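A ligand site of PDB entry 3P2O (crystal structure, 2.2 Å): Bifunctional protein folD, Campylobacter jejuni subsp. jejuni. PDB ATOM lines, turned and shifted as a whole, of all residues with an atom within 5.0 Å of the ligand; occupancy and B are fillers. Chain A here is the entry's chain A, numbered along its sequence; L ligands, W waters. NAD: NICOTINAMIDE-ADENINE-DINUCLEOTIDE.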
ATOM      1  N   THR A 143      -3.576 -35.154  -9.384  1.00  0.00           N
ATOM      2  CA  THR A 143      -2.280 -34.622  -8.989  1.00  0.00           C
ATOM      3  C   THR A 143      -1.908 -35.016  -7.551  1.00  0.00           C
ATOM      4  O   THR A 143      -0.908 -35.713  -7.338  1.00  0.00           O
ATOM      5  CB  THR A 143      -2.201 -33.107  -9.161  1.00  0.00           C
ATOM      6  OG1 THR A 143      -2.416 -32.791 -10.538  1.00  0.00           O
ATOM      7  CG2 THR A 143      -0.795 -32.606  -8.750  1.00  0.00           C
ATOM      8  N   ILE A 166       2.236 -25.713  -0.004  1.00  0.00           N
ATOM      9  CA  ILE A 166       2.224 -24.329  -0.443  1.00  0.00           C
ATOM     10  C   ILE A 166       1.328 -24.164  -1.671  1.00  0.00           C
ATOM     11  O   ILE A 166       1.620 -24.708  -2.738  1.00  0.00           O
ATOM     12  CB  ILE A 166       3.623 -23.792  -0.785  1.00  0.00           C
ATOM     13  CG1 ILE A 166       4.625 -24.061   0.348  1.00  0.00           C
ATOM     14  CG2 ILE A 166       3.553 -22.311  -1.094  1.00  0.00           C
ATOM     15  CD1 ILE A 166       6.104 -23.680  -0.033  1.00  0.00           C
ATOM     16  N   GLY A 167       0.257 -23.394  -1.502  1.00  0.00           N
ATOM     17  CA  GLY A 167      -0.803 -23.351  -2.489  1.00  0.00           C
ATOM     18  C   GLY A 167      -2.056 -24.003  -1.934  1.00  0.00           C
ATOM     19  O   GLY A 167      -1.971 -25.051  -1.281  1.00  0.00           O
ATOM     20  N   ALA A 168      -3.209 -23.382  -2.149  1.00  0.00           N
ATOM     21  CA  ALA A 168      -4.457 -23.895  -1.578  1.00  0.00           C
ATOM     22  C   ALA A 168      -5.625 -24.090  -2.599  1.00  0.00           C
ATOM     23  O   ALA A 168      -6.808 -23.891  -2.256  1.00  0.00           O
ATOM     24  CB  ALA A 168      -4.913 -23.014  -0.394  1.00  0.00           C
ATOM     25  N   SER A 169      -5.300 -24.473  -3.823  1.00  0.00           N
ATOM     26  CA  SER A 169      -6.337 -24.583  -4.855  1.00  0.00           C
ATOM     27  C   SER A 169      -7.163 -25.852  -4.690  1.00  0.00           C
ATOM     28  O   SER A 169      -6.784 -26.792  -3.959  1.00  0.00           O
ATOM     29  CB  SER A 169      -5.737 -24.617  -6.257  1.00  0.00           C
ATOM     30  OG  SER A 169      -5.243 -25.907  -6.498  1.00  0.00           O
ATOM     31  N   ILE A 171      -7.731 -27.864  -7.230  1.00  0.00           N
ATOM     32  CA  ILE A 171      -7.105 -28.867  -8.084  1.00  0.00           C
ATOM     33  C   ILE A 171      -5.978 -29.628  -7.383  1.00  0.00           C
ATOM     34  O   ILE A 171      -5.769 -30.811  -7.631  1.00  0.00           O
ATOM     35  CB  ILE A 171      -6.491 -28.242  -9.341  1.00  0.00           C
ATOM     36  CG1 ILE A 171      -7.493 -27.329 -10.048  1.00  0.00           C
ATOM     37  CG2 ILE A 171      -5.932 -29.321 -10.235  1.00  0.00           C
ATOM     38  CD1 ILE A 171      -8.607 -28.069 -10.704  1.00  0.00           C
ATOM     39  N   VAL A 172      -5.229 -28.934  -6.523  1.00  0.00           N
ATOM     40  CA  VAL A 172      -4.036 -29.530  -5.894  1.00  0.00           C
ATOM     41  C   VAL A 172      -3.988 -29.335  -4.373  1.00  0.00           C
ATOM     42  O   VAL A 172      -4.204 -30.284  -3.620  1.00  0.00           O
ATOM     43  CB  VAL A 172      -2.719 -28.917  -6.454  1.00  0.00           C
ATOM     44  CG1 VAL A 172      -1.547 -29.734  -6.003  1.00  0.00           C
ATOM     45  CG2 VAL A 172      -2.748 -28.869  -7.985  1.00  0.00           C
ATOM     46  N   CYS A 190      -0.419 -23.058   3.286  1.00  0.00           N
ATOM     47  CA  CYS A 190      -0.037 -21.681   3.022  1.00  0.00           C
ATOM     48  C   CYS A 190      -0.462 -21.262   1.632  1.00  0.00           C
ATOM     49  O   CYS A 190      -0.714 -22.088   0.765  1.00  0.00           O
ATOM     50  CB  CYS A 190       1.495 -21.503   3.170  1.00  0.00           C
ATOM     51  SG  CYS A 190       2.179 -22.177   4.724  1.00  0.00           S
ATOM     52  N   HIS A 191      -0.480 -19.959   1.401  1.00  0.00           N
ATOM     53  CA  HIS A 191      -0.896 -19.444   0.119  1.00  0.00           C
ATOM     54  C   HIS A 191      -0.450 -18.008   0.034  1.00  0.00           C
ATOM     55  O   HIS A 191       0.264 -17.525   0.912  1.00  0.00           O
ATOM     56  CB  HIS A 191      -2.420 -19.549   0.016  1.00  0.00           C
ATOM     57  CG  HIS A 191      -3.122 -19.155   1.276  1.00  0.00           C
ATOM     58  ND1 HIS A 191      -3.404 -17.844   1.572  1.00  0.00           N
ATOM     59  CD2 HIS A 191      -3.562 -19.884   2.325  1.00  0.00           C
ATOM     60  CE1 HIS A 191      -4.008 -17.772   2.748  1.00  0.00           C
ATOM     61  NE2 HIS A 191      -4.115 -18.997   3.230  1.00  0.00           N
ATOM     62  N   ILE A 192      -0.911 -17.304  -0.993  1.00  0.00           N
ATOM     63  CA  ILE A 192      -0.378 -15.991  -1.303  1.00  0.00           C
ATOM     64  C   ILE A 192      -0.569 -14.995  -0.150  1.00  0.00           C
ATOM     65  O   ILE A 192       0.172 -14.006  -0.021  1.00  0.00           O
ATOM     66  CB  ILE A 192      -0.975 -15.444  -2.604  1.00  0.00           C
ATOM     67  CG1 ILE A 192      -0.243 -14.178  -3.043  1.00  0.00           C
ATOM     68  CG2 ILE A 192      -2.474 -15.228  -2.469  1.00  0.00           C
ATOM     69  CD1 ILE A 192       0.904 -14.432  -4.031  1.00  0.00           C
ATOM     70  N   LEU A 197       6.309 -17.521   4.824  1.00  0.00           N
ATOM     71  CA  LEU A 197       6.413 -18.924   4.435  1.00  0.00           C
ATOM     72  C   LEU A 197       7.504 -19.708   5.192  1.00  0.00           C
ATOM     73  O   LEU A 197       7.311 -20.896   5.508  1.00  0.00           O
ATOM     74  CB  LEU A 197       6.698 -18.967   2.934  1.00  0.00           C
ATOM     75  CG  LEU A 197       5.886 -19.737   1.911  1.00  0.00           C
ATOM     76  CD1 LEU A 197       4.392 -19.700   2.214  1.00  0.00           C
ATOM     77  CD2 LEU A 197       6.191 -19.148   0.541  1.00  0.00           C
ATOM     78  N   ALA A 210       3.061 -25.893  -4.775  1.00  0.00           N
ATOM     79  CA  ALA A 210       2.097 -25.888  -5.876  1.00  0.00           C
ATOM     80  C   ALA A 210       1.457 -24.534  -6.020  1.00  0.00           C
ATOM     81  O   ALA A 210       0.274 -24.349  -5.719  1.00  0.00           O
ATOM     82  CB  ALA A 210       1.015 -26.970  -5.641  1.00  0.00           C
ATOM     83  N   ALA A 211       2.245 -23.578  -6.510  1.00  0.00           N
ATOM     84  CA  ALA A 211       1.866 -22.183  -6.429  1.00  0.00           C
ATOM     85  C   ALA A 211       1.951 -21.487  -7.763  1.00  0.00           C
ATOM     86  O   ALA A 211       1.347 -20.433  -7.947  1.00  0.00           O
ATOM     87  CB  ALA A 211       2.765 -21.455  -5.433  1.00  0.00           C
ATOM     88  N   GLY A 212       2.730 -22.035  -8.687  1.00  0.00           N
ATOM     89  CA  GLY A 212       2.984 -21.306  -9.931  1.00  0.00           C
ATOM     90  C   GLY A 212       3.823 -20.043  -9.724  1.00  0.00           C
ATOM     91  O   GLY A 212       3.431 -18.939 -10.109  1.00  0.00           O
ATOM     92  N   CYS A 213       4.988 -20.224  -9.110  1.00  0.00           N
ATOM     93  CA  CYS A 213       5.866 -19.100  -8.829  1.00  0.00           C
ATOM     94  C   CYS A 213       7.303 -19.596  -8.841  1.00  0.00           C
ATOM     95  O   CYS A 213       7.670 -20.468  -8.063  1.00  0.00           O
ATOM     96  CB  CYS A 213       5.536 -18.496  -7.474  1.00  0.00           C
ATOM     97  SG  CYS A 213       6.525 -17.052  -7.083  1.00  0.00           S
ATOM     98  N   LEU A 216      10.014 -20.107  -5.621  1.00  0.00           N
ATOM     99  CA  LEU A 216       9.295 -19.783  -4.389  1.00  0.00           C
ATOM    100  C   LEU A 216       9.980 -20.465  -3.196  1.00  0.00           C
ATOM    101  O   LEU A 216       9.941 -19.975  -2.071  1.00  0.00           O
ATOM    102  CB  LEU A 216       7.820 -20.226  -4.494  1.00  0.00           C
ATOM    103  CG  LEU A 216       6.851 -19.888  -3.344  1.00  0.00           C
ATOM    104  CD1 LEU A 216       7.016 -18.422  -2.858  1.00  0.00           C
ATOM    105  CD2 LEU A 216       5.393 -20.176  -3.761  1.00  0.00           C
ATOM    106  N   VAL A 231       5.191 -29.341  -7.592  1.00  0.00           N
ATOM    107  CA  VAL A 231       4.051 -29.552  -8.493  1.00  0.00           C
ATOM    108  C   VAL A 231       3.998 -28.465  -9.549  1.00  0.00           C
ATOM    109  O   VAL A 231       3.349 -28.598 -10.599  1.00  0.00           O
ATOM    110  CB  VAL A 231       2.684 -29.572  -7.737  1.00  0.00           C
ATOM    111  CG1 VAL A 231       1.525 -29.575  -8.718  1.00  0.00           C
ATOM    112  CG2 VAL A 231       2.580 -30.784  -6.823  1.00  0.00           C
ATOM    113  N   GLY A 232       4.684 -27.350  -9.271  1.00  0.00           N
ATOM    114  CA  GLY A 232       4.634 -26.197 -10.146  1.00  0.00           C
ATOM    115  C   GLY A 232       5.087 -26.513 -11.583  1.00  0.00           C
ATOM    116  O   GLY A 232       5.868 -27.439 -11.817  1.00  0.00           O
ATOM    117  N   ILE A 233       4.581 -25.726 -12.526  1.00  0.00           N
ATOM    118  CA  ILE A 233       5.057 -25.795 -13.903  1.00  0.00           C
ATOM    119  C   ILE A 233       5.124 -24.383 -14.446  1.00  0.00           C
ATOM    120  O   ILE A 233       4.101 -23.739 -14.635  1.00  0.00           O
ATOM    121  CB  ILE A 233       4.153 -26.657 -14.780  1.00  0.00           C
ATOM    122  CG1 ILE A 233       4.392 -28.149 -14.476  1.00  0.00           C
ATOM    123  CG2 ILE A 233       4.397 -26.366 -16.263  1.00  0.00           C
ATOM    124  CD1 ILE A 233       3.316 -29.061 -14.996  1.00  0.00           C
ATOM    125  N   ASN A 234       6.349 -23.890 -14.660  1.00  0.00           N
ATOM    126  CA  ASN A 234       6.533 -22.544 -15.198  1.00  0.00           C
ATOM    127  C   ASN A 234       7.467 -22.540 -16.408  1.00  0.00           C
ATOM    128  O   ASN A 234       8.482 -23.239 -16.427  1.00  0.00           O
ATOM    129  CB  ASN A 234       7.033 -21.584 -14.112  1.00  0.00           C
ATOM    130  CG  ASN A 234       6.220 -21.673 -12.800  1.00  0.00           C
ATOM    131  OD1 ASN A 234       5.274 -20.925 -12.575  1.00  0.00           O
ATOM    132  ND2 ASN A 234       6.619 -22.594 -11.939  1.00  0.00           N
ATOM    133  N   ASP A 244       8.411 -24.757  -9.097  1.00  0.00           N
ATOM    134  CA  ASP A 244       8.407 -23.619  -8.177  1.00  0.00           C
ATOM    135  C   ASP A 244       9.599 -23.685  -7.233  1.00  0.00           C
ATOM    136  O   ASP A 244       9.863 -22.736  -6.491  1.00  0.00           O
ATOM    137  CB  ASP A 244       7.139 -23.609  -7.322  1.00  0.00           C
ATOM    138  CG  ASP A 244       5.849 -23.536  -8.145  1.00  0.00           C
ATOM    139  OD1 ASP A 244       5.842 -22.896  -9.227  1.00  0.00           O
ATOM    140  OD2 ASP A 244       4.837 -24.084  -7.663  1.00  0.00           O
ATOM    141  N   VAL A 264       6.066 -34.955 -10.750  1.00  0.00           N
ATOM    142  CA  VAL A 264       4.631 -34.969 -10.509  1.00  0.00           C
ATOM    143  C   VAL A 264       3.843 -35.162 -11.808  1.00  0.00           C
ATOM    144  O   VAL A 264       2.884 -35.952 -11.862  1.00  0.00           O
ATOM    145  CB  VAL A 264       4.182 -33.688  -9.776  1.00  0.00           C
ATOM    146  CG1 VAL A 264       2.681 -33.701  -9.545  1.00  0.00           C
ATOM    147  CG2 VAL A 264       4.944 -33.507  -8.430  1.00  0.00           C
ATOM    148  N   GLY A 265       4.275 -34.460 -12.866  1.00  0.00           N
ATOM    149  CA  GLY A 265       3.620 -34.498 -14.167  1.00  0.00           C
ATOM    150  C   GLY A 265       3.165 -35.863 -14.673  1.00  0.00           C
ATOM    151  O   GLY A 265       1.975 -36.098 -14.807  1.00  0.00           O
ATOM    152  N   THR A 268       0.379 -37.380 -12.356  1.00  0.00           N
ATOM    153  CA  THR A 268      -0.941 -36.849 -12.578  1.00  0.00           C
ATOM    154  C   THR A 268      -1.589 -37.602 -13.739  1.00  0.00           C
ATOM    155  O   THR A 268      -2.718 -38.053 -13.635  1.00  0.00           O
ATOM    156  CB  THR A 268      -0.848 -35.369 -12.918  1.00  0.00           C
ATOM    157  OG1 THR A 268      -0.205 -34.699 -11.832  1.00  0.00           O
ATOM    158  CG2 THR A 268      -2.247 -34.777 -13.125  1.00  0.00           C
HETATM  159  PA  NAD L   1      -3.737 -21.842  -8.633  1.00  0.00           P
HETATM  160  O1A NAD L   1      -5.235 -22.069  -8.729  1.00  0.00           O
HETATM  161  O2A NAD L   1      -3.385 -20.513  -9.254  1.00  0.00           O
HETATM  162  O5B NAD L   1      -3.352 -21.898  -7.115  1.00  0.00           O
HETATM  163  C5B NAD L   1      -2.234 -21.242  -6.609  1.00  0.00           C
HETATM  164  C4B NAD L   1      -2.077 -21.326  -5.154  1.00  0.00           C
HETATM  165  O4B NAD L   1      -0.751 -21.029  -4.794  1.00  0.00           O
HETATM  166  C3B NAD L   1      -2.979 -20.310  -4.544  1.00  0.00           C
HETATM  167  O3B NAD L   1      -3.454 -20.798  -3.316  1.00  0.00           O
HETATM  168  C2B NAD L   1      -2.116 -19.223  -4.387  1.00  0.00           C
HETATM  169  O2B NAD L   1      -2.524 -18.306  -3.416  1.00  0.00           O
HETATM  170  C1B NAD L   1      -0.791 -19.845  -4.086  1.00  0.00           C
HETATM  171  N9A NAD L   1       0.353 -19.002  -4.453  1.00  0.00           N
HETATM  172  C8A NAD L   1       0.577 -18.377  -5.632  1.00  0.00           C
HETATM  173  N7A NAD L   1       1.685 -17.621  -5.541  1.00  0.00           N
HETATM  174  C5A NAD L   1       2.188 -17.775  -4.296  1.00  0.00           C
HETATM  175  C6A NAD L   1       3.296 -17.284  -3.598  1.00  0.00           C
HETATM  176  N6A NAD L   1       4.183 -16.358  -4.215  1.00  0.00           N
HETATM  177  N1A NAD L   1       3.503 -17.641  -2.331  1.00  0.00           N
HETATM  178  C2A NAD L   1       2.672 -18.469  -1.696  1.00  0.00           C
HETATM  179  N3A NAD L   1       1.599 -18.971  -2.328  1.00  0.00           N
HETATM  180  C4A NAD L   1       1.330 -18.646  -3.608  1.00  0.00           C
HETATM  181  O3  NAD L   1      -2.983 -22.972  -9.417  1.00  0.00           O
HETATM  182  PN  NAD L   1      -3.026 -24.566  -9.312  1.00  0.00           P
HETATM  183  O1N NAD L   1      -3.156 -25.014  -7.862  1.00  0.00           O
HETATM  184  O2N NAD L   1      -4.050 -25.188 -10.223  1.00  0.00           O
HETATM  185  O5D NAD L   1      -1.596 -25.056  -9.763  1.00  0.00           O
HETATM  186  C5D NAD L   1      -0.405 -24.524  -9.226  1.00  0.00           C
HETATM  187  C4D NAD L   1       0.835 -24.987  -9.950  1.00  0.00           C
HETATM  188  O4D NAD L   1       0.787 -26.390 -10.163  1.00  0.00           O
HETATM  189  C3D NAD L   1       0.807 -24.330 -11.308  1.00  0.00           C
HETATM  190  O3D NAD L   1       2.131 -24.094 -11.700  1.00  0.00           O
HETATM  191  C2D NAD L   1       0.156 -25.401 -12.195  1.00  0.00           C
HETATM  192  O2D NAD L   1       0.558 -25.277 -13.527  1.00  0.00           O
HETATM  193  C1D NAD L   1       0.743 -26.661 -11.562  1.00  0.00           C
HETATM  194  N1N NAD L   1      -0.038 -27.887 -11.864  1.00  0.00           N
HETATM  195  C2N NAD L   1       0.622 -28.976 -12.373  1.00  0.00           C
HETATM  196  C3N NAD L   1      -0.099 -30.037 -12.932  1.00  0.00           C
HETATM  197  C7N NAD L   1       0.606 -31.046 -13.802  1.00  0.00           C
HETATM  198  O7N NAD L   1      -0.077 -31.713 -14.852  1.00  0.00           O
HETATM  199  N7N NAD L   1       1.878 -31.302 -13.541  1.00  0.00           N
HETATM  200  C4N NAD L   1      -1.424 -30.235 -12.492  1.00  0.00           C
HETATM  201  C5N NAD L   1      -1.975 -29.277 -11.636  1.00  0.00           C
HETATM  202  C6N NAD L   1      -1.363 -28.019 -11.518  1.00  0.00           C
HETATM  203  O   HOH W   1      -2.624 -25.379  -5.175  1.00  0.00           O
HETATM  204  O   HOH W   2      -5.815 -19.554  -2.143  1.00  0.00           O
HETATM  205  O   HOH W   3      -6.944 -21.437  -6.750  1.00  0.00           O
HETATM  206  O   HOH W   4       4.375 -15.591  -0.034  1.00  0.00           O
HETATM  207  O   HOH W   5       2.353 -15.906  -7.493  1.00  0.00           O
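N of Ala 168 is in hydrogen-bond range of O3B of the ligand (2.8 Å).
The side-chain sulfur (SG) of Cys 213 sits at hydrogen-bond distance from a nitrogen (N6A) of the ligand (3.8 Å).
N of Ile 192 sits at hydrogen-bond distance from O2B of the ligand, at 3.1 Å.
An oxygen (O1N) of the ligand lies within hydrogen-bond range of the side-chain hydroxyl of Ser 169, at 2.6 Å.
An oxygen (O3D) of the ligand sits at hydrogen-bond distance from the backbone NH of Ile 233 (3.1 Å).
The backbone NH (N) of Ala 211 sits at hydrogen-bond distance from the side-chain carboxylate (OD2) of Asp 244, 2.9 Å away.
The side-chain hydroxyl (OG) of Ser 169 is in hydrogen-bond range of the backbone NH (N) of Ile 171, at 3.2 Å.
The side-chain hydroxyl (OG1) of Thr 143 sits at hydrogen-bond distance from the side-chain hydroxyl (OG1) of Thr 268 (3.2 Å).
N of Cys 213 is in hydrogen-bond range of OD1 of Asp 244.
The side-chain hydroxyl of Ser 169 is in hydrogen-bond range of the backbone NH of Val 172.
The backbone carbonyl oxygen (O) of Cys 190 is in hydrogen-bond range of the backbone NH (N) of Gly 167 (2.8 Å).
The backbone carbonyl oxygen (O) of Ile 166 sits at hydrogen-bond distance from the backbone NH (N) of Ala 210 (2.8 Å).
The backbone NH (N) of Leu 216 is in hydrogen-bond range of the backbone carbonyl oxygen (O) of Asp 244, 2.8 Å away.
O of Val 231 sits close to O4D of the ligand.
Merely in contact with the ligand: Ala 211, His 191, Gly 167, Thr 143, Gly 212, Leu 216, Ala 210, Gly 232, Gly 265, Val 172 and Ile 166.
Hydrophobic or aromatic side chains that line the ligand: Ile 166, Ala 168, Val 172, His 191, Ile 192, Ala 211, Leu 216, Val 231 and Ile 233.
The nearest printed residue that does not touch the ligand is Ile 171 (4.01 Å).
Water W1 lies within hydrogen-bond range of an oxygen (O1N) of the ligand (2.8 Å), the side-chain hydroxyl of Ser 169 (3.0 Å) and the backbone carbonyl oxygen of Ala 210 (3.1 Å).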
